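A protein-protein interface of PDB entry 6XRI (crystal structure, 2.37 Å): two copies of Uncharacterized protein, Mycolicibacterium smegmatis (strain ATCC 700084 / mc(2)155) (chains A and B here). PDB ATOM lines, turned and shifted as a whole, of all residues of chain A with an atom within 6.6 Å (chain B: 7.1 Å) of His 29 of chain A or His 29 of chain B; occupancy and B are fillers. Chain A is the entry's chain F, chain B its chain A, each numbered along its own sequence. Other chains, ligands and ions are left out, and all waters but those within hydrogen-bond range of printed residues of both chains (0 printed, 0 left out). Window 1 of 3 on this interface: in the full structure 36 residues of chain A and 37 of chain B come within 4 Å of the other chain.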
ATOM      1  N   LEU A  20      12.044  28.091   1.321  1.00  0.00           N
ATOM      2  CA  LEU A  20      11.423  26.785   1.165  1.00  0.00           C
ATOM      3  C   LEU A  20      10.076  26.730   1.858  1.00  0.00           C
ATOM      4  O   LEU A  20       9.147  26.081   1.370  1.00  0.00           O
ATOM      5  CB  LEU A  20      12.330  25.699   1.734  1.00  0.00           C
ATOM      6  CG  LEU A  20      11.750  24.285   1.685  1.00  0.00           C
ATOM      7  CD1 LEU A  20      11.688  23.726   0.260  1.00  0.00           C
ATOM      8  CD2 LEU A  20      12.587  23.366   2.588  1.00  0.00           C
ATOM      9  N   GLY A  23       6.875  28.336   0.090  1.00  0.00           N
ATOM     10  CA  GLY A  23       6.303  27.535  -0.973  1.00  0.00           C
ATOM     11  C   GLY A  23       5.483  26.377  -0.438  1.00  0.00           C
ATOM     12  O   GLY A  23       5.297  25.363  -1.120  1.00  0.00           O
ATOM     13  N   THR A  24       4.996  26.513   0.793  1.00  0.00           N
ATOM     14  CA  THR A  24       4.078  25.551   1.382  1.00  0.00           C
ATOM     15  C   THR A  24       2.863  26.280   1.931  1.00  0.00           C
ATOM     16  O   THR A  24       2.943  27.452   2.307  1.00  0.00           O
ATOM     17  CB  THR A  24       4.713  24.778   2.520  1.00  0.00           C
ATOM     18  OG1 THR A  24       4.898  25.670   3.621  1.00  0.00           O
ATOM     19  CG2 THR A  24       6.072  24.205   2.110  1.00  0.00           C
ATOM     20  N   THR A  25       1.728  25.585   1.953  1.00  0.00           N
ATOM     21  CA  THR A  25       0.559  26.044   2.691  1.00  0.00           C
ATOM     22  C   THR A  25       0.350  25.264   3.978  1.00  0.00           C
ATOM     23  O   THR A  25      -0.456  25.683   4.816  1.00  0.00           O
ATOM     24  CB  THR A  25      -0.704  25.939   1.823  1.00  0.00           C
ATOM     25  OG1 THR A  25      -0.860  24.585   1.383  1.00  0.00           O
ATOM     26  CG2 THR A  25      -0.592  26.859   0.634  1.00  0.00           C
ATOM     27  N   ASP A  26       1.050  24.139   4.146  1.00  0.00           N
ATOM     28  CA  ASP A  26       0.999  23.336   5.357  1.00  0.00           C
ATOM     29  C   ASP A  26       2.334  23.252   6.081  1.00  0.00           C
ATOM     30  O   ASP A  26       2.349  23.022   7.298  1.00  0.00           O
ATOM     31  CB  ASP A  26       0.520  21.909   5.031  1.00  0.00           C
ATOM     32  CG  ASP A  26       1.337  21.253   3.939  1.00  0.00           C
ATOM     33  OD1 ASP A  26       2.324  21.868   3.476  1.00  0.00           O
ATOM     34  OD2 ASP A  26       0.983  20.124   3.544  1.00  0.00           O
ATOM     35  N   GLY A  27       3.441  23.441   5.379  1.00  0.00           N
ATOM     36  CA  GLY A  27       4.756  23.366   5.968  1.00  0.00           C
ATOM     37  C   GLY A  27       5.559  22.165   5.538  1.00  0.00           C
ATOM     38  O   GLY A  27       6.739  22.078   5.899  1.00  0.00           O
ATOM     39  N   VAL A  28       4.967  21.243   4.771  1.00  0.00           N
ATOM     40  CA  VAL A  28       5.640  20.032   4.317  1.00  0.00           C
ATOM     41  C   VAL A  28       5.702  19.940   2.796  1.00  0.00           C
ATOM     42  O   VAL A  28       6.726  19.524   2.246  1.00  0.00           O
ATOM     43  CB  VAL A  28       4.958  18.779   4.902  1.00  0.00           C
ATOM     44  CG1 VAL A  28       5.322  18.623   6.352  1.00  0.00           C
ATOM     45  CG2 VAL A  28       3.439  18.886   4.734  1.00  0.00           C
ATOM     46  N   HIS A  29       4.624  20.301   2.094  1.00  0.00           N
ATOM     47  CA  HIS A  29       4.477  19.995   0.669  1.00  0.00           C
ATOM     48  C   HIS A  29       4.696  21.260  -0.142  1.00  0.00           C
ATOM     49  O   HIS A  29       3.975  22.245   0.044  1.00  0.00           O
ATOM     50  CB  HIS A  29       3.094  19.421   0.331  1.00  0.00           C
ATOM     51  CG  HIS A  29       2.897  18.018   0.802  1.00  0.00           C
ATOM     52  ND1 HIS A  29       2.235  17.704   1.970  1.00  0.00           N
ATOM     53  CD2 HIS A  29       3.314  16.843   0.277  1.00  0.00           C
ATOM     54  CE1 HIS A  29       2.247  16.394   2.140  1.00  0.00           C
ATOM     55  NE2 HIS A  29       2.897  15.849   1.128  1.00  0.00           N
ATOM     56  N   VAL A  30       5.654  21.213  -1.064  1.00  0.00           N
ATOM     57  CA  VAL A  30       5.909  22.307  -1.995  1.00  0.00           C
ATOM     58  C   VAL A  30       5.367  21.902  -3.353  1.00  0.00           C
ATOM     59  O   VAL A  30       5.928  21.031  -4.030  1.00  0.00           O
ATOM     60  CB  VAL A  30       7.397  22.657  -2.075  1.00  0.00           C
ATOM     61  CG1 VAL A  30       7.598  23.812  -3.057  1.00  0.00           C
ATOM     62  CG2 VAL A  30       7.911  22.998  -0.687  1.00  0.00           C
ATOM     63  N   LEU A  31       4.293  22.566  -3.758  1.00  0.00           N
ATOM     64  CA  LEU A  31       3.559  22.225  -4.965  1.00  0.00           C
ATOM     65  C   LEU A  31       3.669  23.321  -6.020  1.00  0.00           C
ATOM     66  O   LEU A  31       3.551  24.514  -5.718  1.00  0.00           O
ATOM     67  CB  LEU A  31       2.085  21.981  -4.639  1.00  0.00           C
ATOM     68  CG  LEU A  31       1.661  20.555  -4.282  1.00  0.00           C
ATOM     69  CD1 LEU A  31       1.912  19.587  -5.413  1.00  0.00           C
ATOM     70  CD2 LEU A  31       2.406  20.117  -3.032  1.00  0.00           C
ATOM     71  N   LEU A  37      -1.922  18.437  -5.162  1.00  0.00           N
ATOM     72  CA  LEU A  37      -1.927  17.479  -4.067  1.00  0.00           C
ATOM     73  C   LEU A  37      -3.343  17.308  -3.542  1.00  0.00           C
ATOM     74  O   LEU A  37      -4.014  18.295  -3.216  1.00  0.00           O
ATOM     75  CB  LEU A  37      -1.003  17.945  -2.953  1.00  0.00           C
ATOM     76  CG  LEU A  37      -0.720  16.921  -1.869  1.00  0.00           C
ATOM     77  CD1 LEU A  37       0.266  15.894  -2.414  1.00  0.00           C
ATOM     78  CD2 LEU A  37      -0.204  17.621  -0.608  1.00  0.00           C
ATOM     79  N   THR A  39      -5.416  15.337  -0.509  1.00  0.00           N
ATOM     80  CA  THR A  39      -5.319  14.656   0.768  1.00  0.00           C
ATOM     81  C   THR A  39      -6.558  13.791   0.939  1.00  0.00           C
ATOM     82  O   THR A  39      -7.683  14.244   0.689  1.00  0.00           O
ATOM     83  CB  THR A  39      -5.172  15.655   1.912  1.00  0.00           C
ATOM     84  OG1 THR A  39      -4.077  16.533   1.632  1.00  0.00           O
ATOM     85  CG2 THR A  39      -4.871  14.933   3.202  1.00  0.00           C
ATOM     86  N   LYS A  48      -4.113  10.747   7.529  1.00  0.00           N
ATOM     87  CA  LYS A  48      -4.089  11.396   6.227  1.00  0.00           C
ATOM     88  C   LYS A  48      -3.004  10.796   5.346  1.00  0.00           C
ATOM     89  O   LYS A  48      -1.851  10.652   5.765  1.00  0.00           O
ATOM     90  CB  LYS A  48      -3.868  12.899   6.376  1.00  0.00           C
ATOM     91  CG  LYS A  48      -5.039  13.659   6.989  1.00  0.00           C
ATOM     92  CD  LYS A  48      -4.546  14.935   7.682  1.00  0.00           C
ATOM     93  CE  LYS A  48      -5.333  15.206   8.990  1.00  0.00           C
ATOM     94  NZ  LYS A  48      -4.494  15.772  10.106  1.00  0.00           N
ATOM     95  N   ARG A  49      -3.395  10.421   4.140  1.00  0.00           N
ATOM     96  CA  ARG A  49      -2.477  10.070   3.077  1.00  0.00           C
ATOM     97  C   ARG A  49      -2.528  11.169   2.035  1.00  0.00           C
ATOM     98  O   ARG A  49      -3.537  11.872   1.906  1.00  0.00           O
ATOM     99  CB  ARG A  49      -2.835   8.725   2.454  1.00  0.00           C
ATOM    100  CG  ARG A  49      -2.239   7.539   3.217  1.00  0.00           C
ATOM    101  CD  ARG A  49      -2.406   7.681   4.724  1.00  0.00           C
ATOM    102  NE  ARG A  49      -2.146   6.409   5.387  1.00  0.00           N
ATOM    103  CZ  ARG A  49      -3.068   5.650   5.981  1.00  0.00           C
ATOM    104  NH1 ARG A  49      -4.343   6.027   6.032  1.00  0.00           N
ATOM    105  NH2 ARG A  49      -2.712   4.500   6.541  1.00  0.00           N
ATOM    106  N   TYR A  50      -1.425  11.312   1.310  1.00  0.00           N
ATOM    107  CA  TYR A  50      -1.259  12.409   0.377  1.00  0.00           C
ATOM    108  C   TYR A  50      -1.113  11.864  -1.037  1.00  0.00           C
ATOM    109  O   TYR A  50      -0.349  10.920  -1.284  1.00  0.00           O
ATOM    110  CB  TYR A  50      -0.078  13.286   0.751  1.00  0.00           C
ATOM    111  CG  TYR A  50      -0.233  13.844   2.148  1.00  0.00           C
ATOM    112  CD1 TYR A  50      -1.053  14.960   2.397  1.00  0.00           C
ATOM    113  CD2 TYR A  50       0.409  13.229   3.234  1.00  0.00           C
ATOM    114  CE1 TYR A  50      -1.198  15.472   3.683  1.00  0.00           C
ATOM    115  CE2 TYR A  50       0.269  13.728   4.525  1.00  0.00           C
ATOM    116  CZ  TYR A  50      -0.534  14.857   4.744  1.00  0.00           C
ATOM    117  OH  TYR A  50      -0.672  15.383   6.016  1.00  0.00           O
ATOM    118  N   VAL A  51      -1.881  12.438  -1.957  1.00  0.00           N
ATOM    119  CA  VAL A  51      -1.930  11.920  -3.327  1.00  0.00           C
ATOM    120  C   VAL A  51      -1.634  13.011  -4.370  1.00  0.00           C
ATOM    121  O   VAL A  51      -2.526  13.799  -4.796  1.00  0.00           O
ATOM    122  CB  VAL A  51      -3.298  11.280  -3.600  1.00  0.00           C
ATOM    123  CG1 VAL A  51      -3.266  10.552  -4.987  1.00  0.00           C
ATOM    124  CG2 VAL A  51      -3.636  10.265  -2.499  1.00  0.00           C
ATOM    125  N   PRO A  52      -0.402  13.043  -4.891  1.00  0.00           N
ATOM    126  CA  PRO A  52      -0.103  13.992  -5.965  1.00  0.00           C
ATOM    127  C   PRO A  52      -0.631  13.433  -7.276  1.00  0.00           C
ATOM    128  O   PRO A  52      -0.437  12.255  -7.587  1.00  0.00           O
ATOM    129  CB  PRO A  52       1.434  14.082  -5.961  1.00  0.00           C
ATOM    130  CG  PRO A  52       1.914  13.237  -4.834  1.00  0.00           C
ATOM    131  CD  PRO A  52       0.798  12.250  -4.569  1.00  0.00           C
ATOM    132  N   GLN A  90      -4.529  20.989  -2.473  1.00  0.00           N
ATOM    133  CA  GLN A  90      -3.506  22.027  -2.507  1.00  0.00           C
ATOM    134  C   GLN A  90      -3.154  22.305  -3.958  1.00  0.00           C
ATOM    135  O   GLN A  90      -2.820  21.374  -4.698  1.00  0.00           O
ATOM    136  CB  GLN A  90      -2.241  21.622  -1.750  1.00  0.00           C
ATOM    137  CG  GLN A  90      -2.394  21.715  -0.253  1.00  0.00           C
ATOM    138  CD  GLN A  90      -1.283  21.052   0.448  1.00  0.00           C
ATOM    139  OE1 GLN A  90      -1.492  20.039   1.083  1.00  0.00           O
ATOM    140  NE2 GLN A  90      -0.081  21.605   0.337  1.00  0.00           N
ATOM    141  N   GLY A  92      -0.577  24.982  -5.668  1.00  0.00           N
ATOM    142  CA  GLY A  92       0.404  26.016  -5.423  1.00  0.00           C
ATOM    143  C   GLY A  92       0.327  26.580  -4.016  1.00  0.00           C
ATOM    144  O   GLY A  92       0.677  25.905  -3.040  1.00  0.00           O
ATOM    145  N   LEU B  20      -4.923   1.255   0.574  1.00  0.00           N
ATOM    146  CA  LEU B  20      -4.222   2.529   0.570  1.00  0.00           C
ATOM    147  C   LEU B  20      -2.823   2.389   1.171  1.00  0.00           C
ATOM    148  O   LEU B  20      -1.809   2.619   0.500  1.00  0.00           O
ATOM    149  CB  LEU B  20      -5.082   3.540   1.338  1.00  0.00           C
ATOM    150  CG  LEU B  20      -4.586   4.957   1.568  1.00  0.00           C
ATOM    151  CD1 LEU B  20      -4.345   5.663   0.280  1.00  0.00           C
ATOM    152  CD2 LEU B  20      -5.612   5.759   2.395  1.00  0.00           C
ATOM    153  N   GLY B  23      -0.280   0.818  -0.930  1.00  0.00           N
ATOM    154  CA  GLY B  23       0.203   1.618  -2.026  1.00  0.00           C
ATOM    155  C   GLY B  23       1.297   2.589  -1.650  1.00  0.00           C
ATOM    156  O   GLY B  23       1.914   3.190  -2.533  1.00  0.00           O
ATOM    157  N   THR B  24       1.589   2.723  -0.375  1.00  0.00           N
ATOM    158  CA  THR B  24       2.639   3.620   0.079  1.00  0.00           C
ATOM    159  C   THR B  24       3.915   2.856   0.421  1.00  0.00           C
ATOM    160  O   THR B  24       3.946   1.624   0.494  1.00  0.00           O
ATOM    161  CB  THR B  24       2.140   4.401   1.290  1.00  0.00           C
ATOM    162  OG1 THR B  24       1.938   3.493   2.375  1.00  0.00           O
ATOM    163  CG2 THR B  24       0.831   5.049   0.967  1.00  0.00           C
ATOM    164  N   THR B  25       4.984   3.624   0.623  1.00  0.00           N
ATOM    165  CA  THR B  25       6.242   3.105   1.136  1.00  0.00           C
ATOM    166  C   THR B  25       6.711   3.829   2.384  1.00  0.00           C
ATOM    167  O   THR B  25       7.630   3.347   3.060  1.00  0.00           O
ATOM    168  CB  THR B  25       7.327   3.203   0.057  1.00  0.00           C
ATOM    169  OG1 THR B  25       7.432   4.562  -0.391  1.00  0.00           O
ATOM    170  CG2 THR B  25       6.957   2.286  -1.109  1.00  0.00           C
ATOM    171  N   ASP B  26       6.129   4.989   2.681  1.00  0.00           N
ATOM    172  CA  ASP B  26       6.357   5.697   3.925  1.00  0.00           C
ATOM    173  C   ASP B  26       5.074   5.807   4.720  1.00  0.00           C
ATOM    174  O   ASP B  26       5.065   6.490   5.744  1.00  0.00           O
ATOM    175  CB  ASP B  26       6.952   7.091   3.674  1.00  0.00           C
ATOM    176  CG  ASP B  26       6.095   7.948   2.800  1.00  0.00           C
ATOM    177  OD1 ASP B  26       5.026   7.512   2.390  1.00  0.00           O
ATOM    178  OD2 ASP B  26       6.485   9.078   2.501  1.00  0.00           O
ATOM    179  N   GLY B  27       3.985   5.191   4.277  1.00  0.00           N
ATOM    180  CA  GLY B  27       2.724   5.258   4.970  1.00  0.00           C
ATOM    181  C   GLY B  27       1.817   6.413   4.582  1.00  0.00           C
ATOM    182  O   GLY B  27       0.620   6.346   4.873  1.00  0.00           O
ATOM    183  N   VAL B  28       2.338   7.485   3.970  1.00  0.00           N
ATOM    184  CA  VAL B  28       1.511   8.671   3.751  1.00  0.00           C
ATOM    185  C   VAL B  28       1.424   9.090   2.297  1.00  0.00           C
ATOM    186  O   VAL B  28       0.433   9.712   1.898  1.00  0.00           O
ATOM    187  CB  VAL B  28       1.990   9.886   4.573  1.00  0.00           C
ATOM    188  CG1 VAL B  28       1.708   9.655   6.065  1.00  0.00           C
ATOM    189  CG2 VAL B  28       3.485  10.242   4.270  1.00  0.00           C
ATOM    190  N   HIS B  29       2.447   8.782   1.499  1.00  0.00           N
ATOM    191  CA  HIS B  29       2.506   9.238   0.111  1.00  0.00           C
ATOM    192  C   HIS B  29       2.149   8.121  -0.864  1.00  0.00           C
ATOM    193  O   HIS B  29       2.857   7.112  -0.960  1.00  0.00           O
ATOM    194  CB  HIS B  29       3.880   9.810  -0.220  1.00  0.00           C
ATOM    195  CG  HIS B  29       4.135  11.123   0.436  1.00  0.00           C
ATOM    196  ND1 HIS B  29       5.024  11.276   1.474  1.00  0.00           N
ATOM    197  CD2 HIS B  29       3.588  12.343   0.224  1.00  0.00           C
ATOM    198  CE1 HIS B  29       5.030  12.533   1.864  1.00  0.00           C
ATOM    199  NE2 HIS B  29       4.170  13.203   1.120  1.00  0.00           N
ATOM    200  N   VAL B  30       1.080   8.340  -1.627  1.00  0.00           N
ATOM    201  CA  VAL B  30       0.620   7.396  -2.646  1.00  0.00           C
ATOM    202  C   VAL B  30       1.174   7.848  -4.014  1.00  0.00           C
ATOM    203  O   VAL B  30       0.757   8.836  -4.601  1.00  0.00           O
ATOM    204  CB  VAL B  30      -0.918   7.273  -2.608  1.00  0.00           C
ATOM    205  CG1 VAL B  30      -1.423   6.193  -3.611  1.00  0.00           C
ATOM    206  CG2 VAL B  30      -1.372   6.949  -1.153  1.00  0.00           C
ATOM    207  N   LEU B  31       2.090   7.233  -4.651  1.00  0.00           N
ATOM    208  CA  LEU B  31       2.596   7.848  -5.867  1.00  0.00           C
ATOM    209  C   LEU B  31       2.266   6.955  -7.039  1.00  0.00           C
ATOM    210  O   LEU B  31       2.493   5.746  -6.954  1.00  0.00           O
ATOM    211  CB  LEU B  31       4.098   8.026  -5.753  1.00  0.00           C
ATOM    212  CG  LEU B  31       4.594   9.387  -5.288  1.00  0.00           C
ATOM    213  CD1 LEU B  31       4.127  10.510  -6.185  1.00  0.00           C
ATOM    214  CD2 LEU B  31       4.157   9.655  -3.857  1.00  0.00           C
ATOM    215  N   LEU B  37       7.995  11.641  -6.182  1.00  0.00           N
ATOM    216  CA  LEU B  37       8.128  12.488  -5.007  1.00  0.00           C
ATOM    217  C   LEU B  37       9.605  12.642  -4.682  1.00  0.00           C
ATOM    218  O   LEU B  37      10.353  11.660  -4.710  1.00  0.00           O
ATOM    219  CB  LEU B  37       7.372  11.892  -3.812  1.00  0.00           C
ATOM    220  CG  LEU B  37       7.233  12.791  -2.581  1.00  0.00           C
ATOM    221  CD1 LEU B  37       6.189  13.873  -2.869  1.00  0.00           C
ATOM    222  CD2 LEU B  37       6.910  11.968  -1.341  1.00  0.00           C
ATOM    223  N   THR B  39      12.113  14.257  -1.642  1.00  0.00           N
ATOM    224  CA  THR B  39      12.143  14.705  -0.254  1.00  0.00           C
ATOM    225  C   THR B  39      13.408  15.523  -0.001  1.00  0.00           C
ATOM    226  O   THR B  39      14.528  15.060  -0.261  1.00  0.00           O
ATOM    227  CB  THR B  39      12.055  13.530   0.726  1.00  0.00           C
ATOM    228  OG1 THR B  39      10.852  12.777   0.507  1.00  0.00           O
ATOM    229  CG2 THR B  39      12.036  14.057   2.171  1.00  0.00           C
ATOM    230  N   LYS B  48      11.914  17.797   7.026  1.00  0.00           N
ATOM    231  CA  LYS B  48      11.624  17.290   5.692  1.00  0.00           C
ATOM    232  C   LYS B  48      10.546  18.125   5.015  1.00  0.00           C
ATOM    233  O   LYS B  48       9.547  18.496   5.632  1.00  0.00           O
ATOM    234  CB  LYS B  48      11.152  15.839   5.755  1.00  0.00           C
ATOM    235  CG  LYS B  48      12.044  14.917   6.526  1.00  0.00           C
ATOM    236  CD  LYS B  48      13.153  14.301   5.696  1.00  0.00           C
ATOM    237  CE  LYS B  48      13.881  13.241   6.537  1.00  0.00           C
ATOM    238  NZ  LYS B  48      15.269  12.996   6.080  1.00  0.00           N
ATOM    239  N   ARG B  49      10.762  18.420   3.742  1.00  0.00           N
ATOM    240  CA  ARG B  49       9.745  18.971   2.864  1.00  0.00           C
ATOM    241  C   ARG B  49       9.594  18.037   1.675  1.00  0.00           C
ATOM    242  O   ARG B  49      10.550  17.367   1.274  1.00  0.00           O
ATOM    243  CB  ARG B  49      10.111  20.378   2.407  1.00  0.00           C
ATOM    244  CG  ARG B  49       9.442  21.453   3.238  1.00  0.00           C
ATOM    245  CD  ARG B  49       9.723  21.296   4.752  1.00  0.00           C
ATOM    246  NE  ARG B  49       9.539  22.575   5.439  1.00  0.00           N
ATOM    247  CZ  ARG B  49      10.513  23.281   6.009  1.00  0.00           C
ATOM    248  NH1 ARG B  49      10.239  24.451   6.578  1.00  0.00           N
ATOM    249  NH2 ARG B  49      11.759  22.820   6.032  1.00  0.00           N
ATOM    250  N   TYR B  50       8.385  17.980   1.130  1.00  0.00           N
ATOM    251  CA  TYR B  50       8.034  17.016   0.099  1.00  0.00           C
ATOM    252  C   TYR B  50       7.657  17.737  -1.183  1.00  0.00           C
ATOM    253  O   TYR B  50       6.801  18.637  -1.185  1.00  0.00           O
ATOM    254  CB  TYR B  50       6.908  16.113   0.587  1.00  0.00           C
ATOM    255  CG  TYR B  50       7.233  15.393   1.891  1.00  0.00           C
ATOM    256  CD1 TYR B  50       8.123  14.328   1.908  1.00  0.00           C
ATOM    257  CD2 TYR B  50       6.649  15.782   3.099  1.00  0.00           C
ATOM    258  CE1 TYR B  50       8.410  13.662   3.067  1.00  0.00           C
ATOM    259  CE2 TYR B  50       6.935  15.122   4.283  1.00  0.00           C
ATOM    260  CZ  TYR B  50       7.817  14.052   4.266  1.00  0.00           C
ATOM    261  OH  TYR B  50       8.117  13.379   5.442  1.00  0.00           O
ATOM    262  N   VAL B  51       8.310  17.329  -2.264  1.00  0.00           N
ATOM    263  CA  VAL B  51       8.204  18.011  -3.547  1.00  0.00           C
ATOM    264  C   VAL B  51       7.760  17.021  -4.611  1.00  0.00           C
ATOM    265  O   VAL B  51       8.590  16.218  -5.088  1.00  0.00           O
ATOM    266  CB  VAL B  51       9.518  18.695  -3.927  1.00  0.00           C
ATOM    267  CG1 VAL B  51       9.332  19.578  -5.174  1.00  0.00           C
ATOM    268  CG2 VAL B  51      10.083  19.526  -2.731  1.00  0.00           C
ATOM    269  N   PRO B  52       6.514  17.050  -5.042  1.00  0.00           N
ATOM    270  CA  PRO B  52       6.093  16.210  -6.170  1.00  0.00           C
ATOM    271  C   PRO B  52       6.428  16.869  -7.505  1.00  0.00           C
ATOM    272  O   PRO B  52       6.109  18.034  -7.748  1.00  0.00           O
ATOM    273  CB  PRO B  52       4.580  16.053  -5.972  1.00  0.00           C
ATOM    274  CG  PRO B  52       4.129  17.093  -4.877  1.00  0.00           C
ATOM    275  CD  PRO B  52       5.426  17.932  -4.555  1.00  0.00           C
ATOM    276  N   SER B  76      10.137  27.246  -4.694  1.00  0.00           N
ATOM    277  CA  SER B  76      10.715  27.498  -3.374  1.00  0.00           C
ATOM    278  C   SER B  76      11.706  26.418  -2.937  1.00  0.00           C
ATOM    279  O   SER B  76      12.446  26.614  -1.968  1.00  0.00           O
ATOM    280  CB  SER B  76       9.592  27.619  -2.356  1.00  0.00           C
ATOM    281  OG  SER B  76       9.128  26.323  -2.044  1.00  0.00           O
ATOM    282  N   GLN B  90      10.801   8.881  -4.247  1.00  0.00           N
ATOM    283  CA  GLN B  90       9.819   7.812  -4.172  1.00  0.00           C
ATOM    284  C   GLN B  90       9.110   7.718  -5.513  1.00  0.00           C
ATOM    285  O   GLN B  90       8.442   8.674  -5.926  1.00  0.00           O
ATOM    286  CB  GLN B  90       8.820   8.084  -3.049  1.00  0.00           C
ATOM    287  CG  GLN B  90       9.477   8.367  -1.682  1.00  0.00           C
ATOM    288  CD  GLN B  90       8.451   8.391  -0.525  1.00  0.00           C
ATOM    289  OE1 GLN B  90       7.350   7.860  -0.658  1.00  0.00           O
ATOM    290  NE2 GLN B  90       8.815   9.009   0.600  1.00  0.00           N
ATOM    291  N   GLY B  92       6.453   5.225  -7.307  1.00  0.00           N
ATOM    292  CA  GLY B  92       5.564   4.087  -7.133  1.00  0.00           C
ATOM    293  C   GLY B  92       5.880   3.378  -5.832  1.00  0.00           C
ATOM    294  O   GLY B  92       5.733   3.941  -4.738  1.00  0.00           O
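NE of Arg 49 of chain A lies within hydrogen-bond range of O of Gly 27 of chain B (2.8 Å). The backbone carbonyl oxygen of Val 28 of chain B is in hydrogen-bond range of the backbone NH of Tyr 50 of chain A (2.5 Å). A ring nitrogen (NE2) of His 29 of chain B is in hydrogen-bond range of a ring nitrogen (NE2) of His 29 of chain A, 2.9 Å away. The backbone carbonyl oxygen (O) of Tyr 50 of chain A is in hydrogen-bond range of the backbone NH (N) of Val 30 of chain B (3.0 Å). The guanidinium group (NE) of Arg 49 of chain B sits at hydrogen-bond distance from the backbone carbonyl oxygen (O) of Gly 27 of chain A (2.9 Å). N of Tyr 50 of chain B is in hydrogen-bond range of O of Val 28 of chain A (2.5 Å). O of Tyr 50 of chain B is in hydrogen-bond range of N of Val 30 of chain A (2.8 Å). The side-chain hydroxyl of Ser 76 of chain B sits at hydrogen-bond distance from the backbone carbonyl oxygen of Leu 20 of chain A, at 3.4 Å.
Printed residues of chain B within 4 Å of His 29 of chain A: His 29 and Tyr 50. His 29 of chain B touches just these residues of chain A: His 29 and Tyr 50. Printed residues of chain B within 4 Å of Leu 31 of chain A: Pro 52 (3.4 Å). Printed residues of chain B within 4 Å of Val 30 of chain A: Tyr 50, Val 51, Pro 52 and Ser 76. Of the printed residues of chain A, Leu 31 of chain B touches Pro 52. Of the printed residues of chain B, Lys 48 of chain A touches Val 28. Leu 37 of chain B touches none of the printed residues of chain A. Gly 23 of chain B touches none of the printed residues of chain A. The nearest printed residue of chain A that does not touch Val 30 of chain B is Val 51 of chain A (4.04 Å).
Val 28 of chain A touches Arg 49 of chain B, and with the chains exchanged Arg 49 of chain A touches Val 28 of chain B. His 29 of chain A touches Tyr 50 of chain B, and with the chains exchanged Tyr 50 of chain A touches His 29 of chain B. Val 30 of chain A touches Tyr 50 of chain B, and with the chains exchanged Tyr 50 of chain A touches Val 30 of chain B. 19 positions are printed for both chains. Of the 23 pairs that touch across the chains among the printed residues, 18 have their exchanged pair printed and touching as well.
Hydrophobic or aromatic side chains of chain B within 4 Å of the printed part of chain A: Leu 20, Val 28, His 29, Val 30, Leu 31, Tyr 50, Val 51 and Pro 52. Printed residues of chain A that touch a printed residue of chain B: Leu 20, Gly 23, Gly 27, Val 28, His 29, Val 30, Leu 31, Lys 48, Arg 49, Tyr 50 and Pro 52. Hydrophobic or aromatic side chains of chain A that line the printed part of chain B: Leu 20, Val 28, His 29, Val 30, Leu 31, Tyr 50 and Pro 52. Among the printed residues, no Asp or Glu carboxylate lies within 4 Å of a Lys or Arg side-chain nitrogen of the other chain.
Among the printed residues, merely in contact across the chains: Leu 20 of chain A with Arg 49 of chain B (3.6 Å), Gly 23 of chain A with Ser 76 of chain B (3.3 Å), Val 28 of chain A with Arg 49 of chain B (3.1 Å), His 29 of chain A with Tyr 50 of chain B (3.3 Å), Val 30 of chain A with Val 51 of chain B (3.8 Å), Val 30 of chain A with Pro 52 of chain B (3.2 Å), Val 30 of chain A with Ser 76 of chain B (3.1 Å), Leu 31 of chain A with Pro 52 of chain B (3.4 Å), Lys 48 of chain A with Val 28 of chain B (3.7 Å), Arg 49 of chain A with Leu 20 of chain B (3.9 Å), Arg 49 of chain A with Val 28 of chain B (3.2 Å), Tyr 50 of chain A with His 29 of chain B (3.6 Å), Pro 52 of chain A with Val 30 of chain B (3.4 Å), Pro 52 of chain A with Leu 31 of chain B (3.8 Å) and Pro 52 of chain A with Pro 52 of chain B (3.7 Å).
The backbone NH (N) of Gly 27 of chain B sits close to the side-chain hydroxyl (OG1) of Thr 24 of chain B, at 3.3 Å. A ring nitrogen (ND1) of His 29 of chain B lies within hydrogen-bond range of the side-chain carboxylate of Asp 26 of chain B (2.8 Å). The backbone NH of Gly 27 of chain A sits at hydrogen-bond distance from the side-chain hydroxyl of Thr 24 of chain A (3.2 Å). The side-chain carboxylate (OD1) of Asp 26 of chain A lies within hydrogen-bond range of the backbone NH (N) of Val 28 of chain A, 3.0 Å away.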
